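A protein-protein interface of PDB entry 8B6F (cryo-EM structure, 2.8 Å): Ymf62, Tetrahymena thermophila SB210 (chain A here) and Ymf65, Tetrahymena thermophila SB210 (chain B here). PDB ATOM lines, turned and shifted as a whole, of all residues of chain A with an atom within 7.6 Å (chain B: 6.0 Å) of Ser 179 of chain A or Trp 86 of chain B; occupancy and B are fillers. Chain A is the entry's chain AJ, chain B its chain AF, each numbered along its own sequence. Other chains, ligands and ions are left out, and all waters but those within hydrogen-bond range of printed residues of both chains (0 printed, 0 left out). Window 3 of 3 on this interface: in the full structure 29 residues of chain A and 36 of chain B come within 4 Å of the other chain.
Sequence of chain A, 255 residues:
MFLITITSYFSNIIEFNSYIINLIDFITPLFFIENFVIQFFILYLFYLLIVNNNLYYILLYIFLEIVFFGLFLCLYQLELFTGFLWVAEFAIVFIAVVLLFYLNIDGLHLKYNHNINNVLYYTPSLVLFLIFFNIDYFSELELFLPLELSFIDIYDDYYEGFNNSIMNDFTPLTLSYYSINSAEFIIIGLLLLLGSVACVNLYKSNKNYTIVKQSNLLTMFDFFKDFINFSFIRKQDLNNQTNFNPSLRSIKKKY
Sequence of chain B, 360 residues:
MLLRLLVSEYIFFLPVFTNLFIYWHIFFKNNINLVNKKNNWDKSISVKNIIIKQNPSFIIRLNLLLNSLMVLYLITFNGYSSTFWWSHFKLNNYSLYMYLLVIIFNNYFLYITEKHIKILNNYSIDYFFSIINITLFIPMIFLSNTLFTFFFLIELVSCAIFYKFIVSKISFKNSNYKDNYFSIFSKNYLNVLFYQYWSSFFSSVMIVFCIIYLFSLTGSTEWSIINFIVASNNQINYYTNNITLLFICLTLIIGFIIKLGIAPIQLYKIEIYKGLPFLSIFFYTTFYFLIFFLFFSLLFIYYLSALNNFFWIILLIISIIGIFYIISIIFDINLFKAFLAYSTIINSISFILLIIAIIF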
ATOM      1  N   PRO A 172     -30.598 -24.462 -19.822  1.00  0.00           N
ATOM      2  CA  PRO A 172     -30.282 -25.086 -21.117  1.00  0.00           C
ATOM      3  C   PRO A 172     -29.610 -24.130 -22.082  1.00  0.00           C
ATOM      4  O   PRO A 172     -28.718 -24.535 -22.835  1.00  0.00           O
ATOM      5  CB  PRO A 172     -31.654 -25.546 -21.630  1.00  0.00           C
ATOM      6  CG  PRO A 172     -32.514 -25.614 -20.426  1.00  0.00           C
ATOM      7  CD  PRO A 172     -32.040 -24.520 -19.530  1.00  0.00           C
ATOM      8  N   LEU A 173     -30.023 -22.862 -22.085  1.00  0.00           N
ATOM      9  CA  LEU A 173     -29.436 -21.900 -23.010  1.00  0.00           C
ATOM     10  C   LEU A 173     -27.957 -21.681 -22.718  1.00  0.00           C
ATOM     11  O   LEU A 173     -27.140 -21.610 -23.643  1.00  0.00           O
ATOM     12  CB  LEU A 173     -30.209 -20.584 -22.940  1.00  0.00           C
ATOM     13  CG  LEU A 173     -31.672 -20.666 -23.390  1.00  0.00           C
ATOM     14  CD1 LEU A 173     -32.379 -19.343 -23.162  1.00  0.00           C
ATOM     15  CD2 LEU A 173     -31.781 -21.079 -24.850  1.00  0.00           C
ATOM     16  N   THR A 174     -27.590 -21.564 -21.440  1.00  0.00           N
ATOM     17  CA  THR A 174     -26.180 -21.391 -21.098  1.00  0.00           C
ATOM     18  C   THR A 174     -25.388 -22.666 -21.353  1.00  0.00           C
ATOM     19  O   THR A 174     -24.258 -22.611 -21.852  1.00  0.00           O
ATOM     20  CB  THR A 174     -26.028 -20.939 -19.643  1.00  0.00           C
ATOM     21  OG1 THR A 174     -24.637 -20.779 -19.333  1.00  0.00           O
ATOM     22  CG2 THR A 174     -26.632 -21.940 -18.685  1.00  0.00           C
ATOM     23  N   LEU A 175     -25.955 -23.824 -21.012  1.00  0.00           N
ATOM     24  CA  LEU A 175     -25.270 -25.084 -21.282  1.00  0.00           C
ATOM     25  C   LEU A 175     -25.050 -25.300 -22.768  1.00  0.00           C
ATOM     26  O   LEU A 175     -24.135 -26.032 -23.161  1.00  0.00           O
ATOM     27  CB  LEU A 175     -26.072 -26.248 -20.703  1.00  0.00           C
ATOM     28  CG  LEU A 175     -25.860 -26.537 -19.222  1.00  0.00           C
ATOM     29  CD1 LEU A 175     -26.941 -27.453 -18.691  1.00  0.00           C
ATOM     30  CD2 LEU A 175     -24.492 -27.165 -19.037  1.00  0.00           C
ATOM     31  N   SER A 176     -25.880 -24.692 -23.609  1.00  0.00           N
ATOM     32  CA  SER A 176     -25.710 -24.806 -25.049  1.00  0.00           C
ATOM     33  C   SER A 176     -24.747 -23.772 -25.620  1.00  0.00           C
ATOM     34  O   SER A 176     -23.795 -24.126 -26.321  1.00  0.00           O
ATOM     35  CB  SER A 176     -27.057 -24.671 -25.744  1.00  0.00           C
ATOM     36  OG  SER A 176     -26.865 -24.867 -27.123  1.00  0.00           O
ATOM     37  N   TYR A 177     -24.978 -22.495 -25.323  1.00  0.00           N
ATOM     38  CA  TYR A 177     -24.212 -21.429 -25.954  1.00  0.00           C
ATOM     39  C   TYR A 177     -22.806 -21.320 -25.388  1.00  0.00           C
ATOM     40  O   TYR A 177     -21.886 -20.919 -26.109  1.00  0.00           O
ATOM     41  CB  TYR A 177     -24.939 -20.092 -25.804  1.00  0.00           C
ATOM     42  CG  TYR A 177     -26.322 -20.073 -26.408  1.00  0.00           C
ATOM     43  CD1 TYR A 177     -26.561 -20.626 -27.659  1.00  0.00           C
ATOM     44  CD2 TYR A 177     -27.392 -19.510 -25.726  1.00  0.00           C
ATOM     45  CE1 TYR A 177     -27.822 -20.615 -28.216  1.00  0.00           C
ATOM     46  CE2 TYR A 177     -28.657 -19.492 -26.277  1.00  0.00           C
ATOM     47  CZ  TYR A 177     -28.866 -20.045 -27.522  1.00  0.00           C
ATOM     48  OH  TYR A 177     -30.125 -20.037 -28.072  1.00  0.00           O
ATOM     49  N   TYR A 178     -22.614 -21.657 -24.116  1.00  0.00           N
ATOM     50  CA  TYR A 178     -21.344 -21.422 -23.451  1.00  0.00           C
ATOM     51  C   TYR A 178     -20.619 -22.697 -23.049  1.00  0.00           C
ATOM     52  O   TYR A 178     -19.451 -22.618 -22.654  1.00  0.00           O
ATOM     53  CB  TYR A 178     -21.562 -20.546 -22.209  1.00  0.00           C
ATOM     54  CG  TYR A 178     -22.090 -19.175 -22.554  1.00  0.00           C
ATOM     55  CD1 TYR A 178     -23.443 -18.969 -22.785  1.00  0.00           C
ATOM     56  CD2 TYR A 178     -21.234 -18.089 -22.666  1.00  0.00           C
ATOM     57  CE1 TYR A 178     -23.932 -17.723 -23.111  1.00  0.00           C
ATOM     58  CE2 TYR A 178     -21.712 -16.836 -22.993  1.00  0.00           C
ATOM     59  CZ  TYR A 178     -23.062 -16.660 -23.215  1.00  0.00           C
ATOM     60  OH  TYR A 178     -23.547 -15.415 -23.537  1.00  0.00           O
ATOM     61  N   SER A 179     -21.264 -23.861 -23.129  1.00  0.00           N
ATOM     62  CA  SER A 179     -20.597 -25.120 -22.817  1.00  0.00           C
ATOM     63  C   SER A 179     -20.514 -26.043 -24.026  1.00  0.00           C
ATOM     64  O   SER A 179     -19.412 -26.459 -24.395  1.00  0.00           O
ATOM     65  CB  SER A 179     -21.316 -25.817 -21.654  1.00  0.00           C
ATOM     66  OG  SER A 179     -20.641 -27.005 -21.279  1.00  0.00           O
ATOM     67  N   ILE A 180     -21.637 -26.365 -24.668  1.00  0.00           N
ATOM     68  CA  ILE A 180     -21.659 -27.395 -25.704  1.00  0.00           C
ATOM     69  C   ILE A 180     -21.507 -26.773 -27.086  1.00  0.00           C
ATOM     70  O   ILE A 180     -20.587 -27.121 -27.835  1.00  0.00           O
ATOM     71  CB  ILE A 180     -22.951 -28.230 -25.625  1.00  0.00           C
ATOM     72  CG1 ILE A 180     -23.063 -28.925 -24.263  1.00  0.00           C
ATOM     73  CG2 ILE A 180     -23.004 -29.255 -26.755  1.00  0.00           C
ATOM     74  CD1 ILE A 180     -21.944 -29.907 -23.961  1.00  0.00           C
ATOM     75  N   ASN A 181     -22.409 -25.855 -27.437  1.00  0.00           N
ATOM     76  CA  ASN A 181     -22.400 -25.212 -28.746  1.00  0.00           C
ATOM     77  C   ASN A 181     -21.619 -23.908 -28.745  1.00  0.00           C
ATOM     78  O   ASN A 181     -21.922 -23.004 -29.534  1.00  0.00           O
ATOM     79  CB  ASN A 181     -23.831 -24.973 -29.226  1.00  0.00           C
ATOM     80  CG  ASN A 181     -24.655 -26.244 -29.255  1.00  0.00           C
ATOM     81  OD1 ASN A 181     -25.355 -26.570 -28.297  1.00  0.00           O
ATOM     82  ND2 ASN A 181     -24.571 -26.971 -30.361  1.00  0.00           N
ATOM     83  N   SER A 182     -20.614 -23.794 -27.880  1.00  0.00           N
ATOM     84  CA  SER A 182     -19.801 -22.586 -27.837  1.00  0.00           C
ATOM     85  C   SER A 182     -19.101 -22.334 -29.165  1.00  0.00           C
ATOM     86  O   SER A 182     -18.841 -21.180 -29.517  1.00  0.00           O
ATOM     87  CB  SER A 182     -18.794 -22.688 -26.696  1.00  0.00           C
ATOM     88  OG  SER A 182     -18.163 -23.954 -26.692  1.00  0.00           O
ATOM     89  N   ALA A 183     -18.795 -23.392 -29.917  1.00  0.00           N
ATOM     90  CA  ALA A 183     -18.216 -23.203 -31.241  1.00  0.00           C
ATOM     91  C   ALA A 183     -19.163 -22.414 -32.133  1.00  0.00           C
ATOM     92  O   ALA A 183     -18.753 -21.467 -32.813  1.00  0.00           O
ATOM     93  CB  ALA A 183     -17.884 -24.557 -31.867  1.00  0.00           C
ATOM     94  N   PHE A 185     -21.555 -20.522 -31.041  1.00  0.00           N
ATOM     95  CA  PHE A 185     -21.662 -19.202 -30.431  1.00  0.00           C
ATOM     96  C   PHE A 185     -20.578 -18.272 -30.965  1.00  0.00           C
ATOM     97  O   PHE A 185     -20.856 -17.131 -31.349  1.00  0.00           O
ATOM     98  CB  PHE A 185     -21.570 -19.338 -28.910  1.00  0.00           C
ATOM     99  CG  PHE A 185     -21.744 -18.047 -28.167  1.00  0.00           C
ATOM    100  CD1 PHE A 185     -22.994 -17.467 -28.044  1.00  0.00           C
ATOM    101  CD2 PHE A 185     -20.663 -17.432 -27.558  1.00  0.00           C
ATOM    102  CE1 PHE A 185     -23.159 -16.285 -27.350  1.00  0.00           C
ATOM    103  CE2 PHE A 185     -20.821 -16.252 -26.862  1.00  0.00           C
ATOM    104  CZ  PHE A 185     -22.072 -15.677 -26.757  1.00  0.00           C
ATOM    105  N   LEU B   2     -17.521 -29.120 -14.905  1.00  0.00           N
ATOM    106  CA  LEU B   2     -16.220 -29.030 -15.622  1.00  0.00           C
ATOM    107  C   LEU B   2     -15.111 -28.691 -14.639  1.00  0.00           C
ATOM    108  O   LEU B   2     -15.165 -27.667 -13.961  1.00  0.00           O
ATOM    109  CB  LEU B   2     -16.286 -27.986 -16.741  1.00  0.00           C
ATOM    110  CG  LEU B   2     -15.014 -27.801 -17.576  1.00  0.00           C
ATOM    111  CD1 LEU B   2     -15.359 -27.507 -19.025  1.00  0.00           C
ATOM    112  CD2 LEU B   2     -14.150 -26.684 -17.010  1.00  0.00           C
ATOM    113  N   LEU B   5      -9.783 -28.509 -18.236  1.00  0.00           N
ATOM    114  CA  LEU B   5      -9.949 -28.168 -19.645  1.00  0.00           C
ATOM    115  C   LEU B   5      -8.691 -28.619 -20.378  1.00  0.00           C
ATOM    116  O   LEU B   5      -7.657 -27.946 -20.329  1.00  0.00           O
ATOM    117  CB  LEU B   5     -10.197 -26.674 -19.822  1.00  0.00           C
ATOM    118  CG  LEU B   5     -10.413 -26.217 -21.266  1.00  0.00           C
ATOM    119  CD1 LEU B   5     -11.683 -26.820 -21.848  1.00  0.00           C
ATOM    120  CD2 LEU B   5     -10.454 -24.706 -21.345  1.00  0.00           C
ATOM    121  N   GLU B   9      -8.663 -30.237 -26.531  1.00  0.00           N
ATOM    122  CA  GLU B   9      -9.942 -29.737 -27.018  1.00  0.00           C
ATOM    123  C   GLU B   9      -9.798 -28.482 -27.869  1.00  0.00           C
ATOM    124  O   GLU B   9     -10.684 -28.199 -28.681  1.00  0.00           O
ATOM    125  CB  GLU B   9     -10.872 -29.443 -25.839  1.00  0.00           C
ATOM    126  CG  GLU B   9     -11.192 -30.653 -24.974  1.00  0.00           C
ATOM    127  CD  GLU B   9     -12.074 -31.666 -25.681  1.00  0.00           C
ATOM    128  OE1 GLU B   9     -12.563 -31.364 -26.789  1.00  0.00           O
ATOM    129  OE2 GLU B   9     -12.282 -32.765 -25.127  1.00  0.00           O
ATOM    130  N   THR B  83     -12.148 -36.613 -32.220  1.00  0.00           N
ATOM    131  CA  THR B  83     -12.888 -35.363 -32.259  1.00  0.00           C
ATOM    132  C   THR B  83     -12.488 -34.487 -31.081  1.00  0.00           C
ATOM    133  O   THR B  83     -12.073 -34.983 -30.032  1.00  0.00           O
ATOM    134  CB  THR B  83     -14.397 -35.615 -32.222  1.00  0.00           C
ATOM    135  OG1 THR B  83     -14.763 -36.186 -30.960  1.00  0.00           O
ATOM    136  CG2 THR B  83     -14.812 -36.556 -33.337  1.00  0.00           C
ATOM    137  N   PHE B  84     -12.616 -33.174 -31.262  1.00  0.00           N
ATOM    138  CA  PHE B  84     -12.245 -32.226 -30.224  1.00  0.00           C
ATOM    139  C   PHE B  84     -13.318 -31.154 -30.092  1.00  0.00           C
ATOM    140  O   PHE B  84     -14.079 -30.883 -31.023  1.00  0.00           O
ATOM    141  CB  PHE B  84     -10.875 -31.586 -30.505  1.00  0.00           C
ATOM    142  CG  PHE B  84     -10.821 -30.776 -31.770  1.00  0.00           C
ATOM    143  CD1 PHE B  84     -10.638 -31.392 -32.995  1.00  0.00           C
ATOM    144  CD2 PHE B  84     -10.929 -29.396 -31.728  1.00  0.00           C
ATOM    145  CE1 PHE B  84     -10.578 -30.648 -34.157  1.00  0.00           C
ATOM    146  CE2 PHE B  84     -10.871 -28.647 -32.885  1.00  0.00           C
ATOM    147  CZ  PHE B  84     -10.695 -29.273 -34.101  1.00  0.00           C
ATOM    148  N   TRP B  85     -13.354 -30.541 -28.910  1.00  0.00           N
ATOM    149  CA  TRP B  85     -14.318 -29.495 -28.570  1.00  0.00           C
ATOM    150  C   TRP B  85     -15.758 -30.004 -28.673  1.00  0.00           C
ATOM    151  O   TRP B  85     -16.554 -29.549 -29.495  1.00  0.00           O
ATOM    152  CB  TRP B  85     -14.111 -28.255 -29.444  1.00  0.00           C
ATOM    153  CG  TRP B  85     -14.780 -27.050 -28.874  1.00  0.00           C
ATOM    154  CD1 TRP B  85     -15.875 -26.408 -29.365  1.00  0.00           C
ATOM    155  CD2 TRP B  85     -14.403 -26.351 -27.683  1.00  0.00           C
ATOM    156  NE1 TRP B  85     -16.201 -25.345 -28.557  1.00  0.00           N
ATOM    157  CE2 TRP B  85     -15.311 -25.290 -27.517  1.00  0.00           C
ATOM    158  CE3 TRP B  85     -13.381 -26.519 -26.743  1.00  0.00           C
ATOM    159  CZ2 TRP B  85     -15.227 -24.397 -26.452  1.00  0.00           C
ATOM    160  CZ3 TRP B  85     -13.300 -25.632 -25.684  1.00  0.00           C
ATOM    161  CH2 TRP B  85     -14.218 -24.585 -25.547  1.00  0.00           C
ATOM    162  N   TRP B  86     -16.079 -30.969 -27.811  1.00  0.00           N
ATOM    163  CA  TRP B  86     -17.440 -31.473 -27.654  1.00  0.00           C
ATOM    164  C   TRP B  86     -17.905 -32.262 -28.872  1.00  0.00           C
ATOM    165  O   TRP B  86     -19.093 -32.269 -29.198  1.00  0.00           O
ATOM    166  CB  TRP B  86     -18.424 -30.335 -27.363  1.00  0.00           C
ATOM    167  CG  TRP B  86     -17.942 -29.395 -26.310  1.00  0.00           C
ATOM    168  CD1 TRP B  86     -17.411 -28.154 -26.503  1.00  0.00           C
ATOM    169  CD2 TRP B  86     -17.934 -29.620 -24.898  1.00  0.00           C
ATOM    170  NE1 TRP B  86     -17.077 -27.592 -25.297  1.00  0.00           N
ATOM    171  CE2 TRP B  86     -17.386 -28.473 -24.296  1.00  0.00           C
ATOM    172  CE3 TRP B  86     -18.338 -30.683 -24.083  1.00  0.00           C
ATOM    173  CZ2 TRP B  86     -17.234 -28.353 -22.918  1.00  0.00           C
ATOM    174  CZ3 TRP B  86     -18.186 -30.564 -22.714  1.00  0.00           C
ATOM    175  CH2 TRP B  86     -17.639 -29.406 -22.145  1.00  0.00           C
ATOM    176  N   SER B  87     -16.978 -32.932 -29.550  1.00  0.00           N
ATOM    177  CA  SER B  87     -17.286 -33.756 -30.714  1.00  0.00           C
ATOM    178  C   SER B  87     -17.901 -32.949 -31.848  1.00  0.00           C
ATOM    179  O   SER B  87     -18.619 -33.501 -32.687  1.00  0.00           O
ATOM    180  CB  SER B  87     -18.216 -34.916 -30.339  1.00  0.00           C
ATOM    181  OG  SER B  87     -17.624 -35.749 -29.355  1.00  0.00           O
ATOM    182  N   HIS B  88     -17.636 -31.645 -31.892  1.00  0.00           N
ATOM    183  CA  HIS B  88     -18.120 -30.810 -32.981  1.00  0.00           C
ATOM    184  C   HIS B  88     -17.139 -30.721 -34.137  1.00  0.00           C
ATOM    185  O   HIS B  88     -17.538 -30.329 -35.237  1.00  0.00           O
ATOM    186  CB  HIS B  88     -18.427 -29.401 -32.467  1.00  0.00           C
ATOM    187  CG  HIS B  88     -19.740 -29.296 -31.756  1.00  0.00           C
ATOM    188  ND1 HIS B  88     -20.140 -30.201 -30.796  1.00  0.00           N
ATOM    189  CD2 HIS B  88     -20.746 -28.400 -31.870  1.00  0.00           C
ATOM    190  CE1 HIS B  88     -21.335 -29.863 -30.347  1.00  0.00           C
ATOM    191  NE2 HIS B  88     -21.726 -28.773 -30.982  1.00  0.00           N
ATOM    192  N   PHE B  89     -15.876 -31.080 -33.922  1.00  0.00           N
ATOM    193  CA  PHE B  89     -14.867 -31.072 -34.969  1.00  0.00           C
ATOM    194  C   PHE B  89     -14.153 -32.412 -34.991  1.00  0.00           C
ATOM    195  O   PHE B  89     -13.844 -32.977 -33.938  1.00  0.00           O
ATOM    196  CB  PHE B  89     -13.856 -29.943 -34.759  1.00  0.00           C
ATOM    197  CG  PHE B  89     -14.445 -28.572 -34.896  1.00  0.00           C
ATOM    198  CD1 PHE B  89     -14.997 -27.930 -33.801  1.00  0.00           C
ATOM    199  CD2 PHE B  89     -14.447 -27.927 -36.119  1.00  0.00           C
ATOM    200  CE1 PHE B  89     -15.539 -26.668 -33.925  1.00  0.00           C
ATOM    201  CE2 PHE B  89     -14.987 -26.667 -36.250  1.00  0.00           C
ATOM    202  CZ  PHE B  89     -15.536 -26.036 -35.152  1.00  0.00           C
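The side-chain amide nitrogen (ND2) of Asn 181 of chain A lies within hydrogen-bond range of a ring nitrogen (NE2) of His 88 of chain B, at 3.4 Å.
The indole nitrogen (NE1) of Trp 85 of chain B sits close to the side-chain hydroxyl (OG) of Ser 182 of chain A, at 3.0 Å.
The indole nitrogen of Trp 86 of chain B lies within hydrogen-bond range of the backbone carbonyl oxygen of Ser 179 of chain A (2.7 Å).
The backbone NH of Phe 84 of chain B is in hydrogen-bond range of the backbone carbonyl oxygen of Phe 89 of chain B.
The backbone NH (N) of Ser 179 of chain A is in hydrogen-bond range of the backbone carbonyl oxygen (O) of Thr 174 of chain A.
The side-chain carboxylate (OE1) of Glu 9 of chain B is in hydrogen-bond range of the backbone NH (N) of Trp 85 of chain B (2.4 Å).
The backbone carbonyl oxygen of Trp 86 of chain B sits at hydrogen-bond distance from a ring nitrogen (ND1) of His 88 of chain B (2.8 Å).
The backbone carbonyl oxygen of Leu 175 of chain A is in hydrogen-bond range of the backbone NH of Ile 180 of chain A.
The backbone carbonyl oxygen of Ser 176 of chain A is in hydrogen-bond range of the backbone NH of Asn 181 of chain A, 2.5 Å away.
Among the printed residues, pairs that only touch across the chains: Ala 183 of chain A with Trp 85 of chain B (3.5 Å), Ile 180 of chain A with Trp 86 of chain B (3.6 Å), Ile 180 of chain A with His 88 of chain B (3.7 Å) and Ala 183 of chain A with Phe 89 of chain B (3.8 Å).
Trp 86 of chain B touches just these residues of chain A: Ser 179 and Ile 180.
Printed residues of chain B within 4 Å of Ala 183 of chain A: Trp 85 (3.5 Å) and Phe 89 (3.8 Å).
Of the printed residues of chain B, Ile 180 of chain A touches Trp 86 (3.6 Å) and His 88 (3.7 Å).
Of the printed residues of chain A, Phe 89 of chain B touches Ala 183.
Printed residues of chain B within 4 Å of Ser 182 of chain A: Trp 85.
Printed residues of chain A within 4 Å of Trp 85 of chain B: Ser 182 and Ala 183.
The nearest residue of chain B that does not touch Ser 179 of chain A is Trp 85 of chain B (5.1 Å).
The nearest residue of chain A that does not touch Trp 86 of chain B is Ser 182 of chain A (4.04 Å).
The nearest printed residue of chain A that does not touch His 88 of chain B is Ala 183 of chain A (4.8 Å).
Of the 13 printed residues of chain A, 5 touch a printed residue of chain B.
Hydrophobic or aromatic side chains of chain A that line the printed part of chain B: Ile 180 and Ala 183.
Printed residues of chain B that touch a printed residue of chain A: Trp 85, Trp 86, His 88 and Phe 89.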
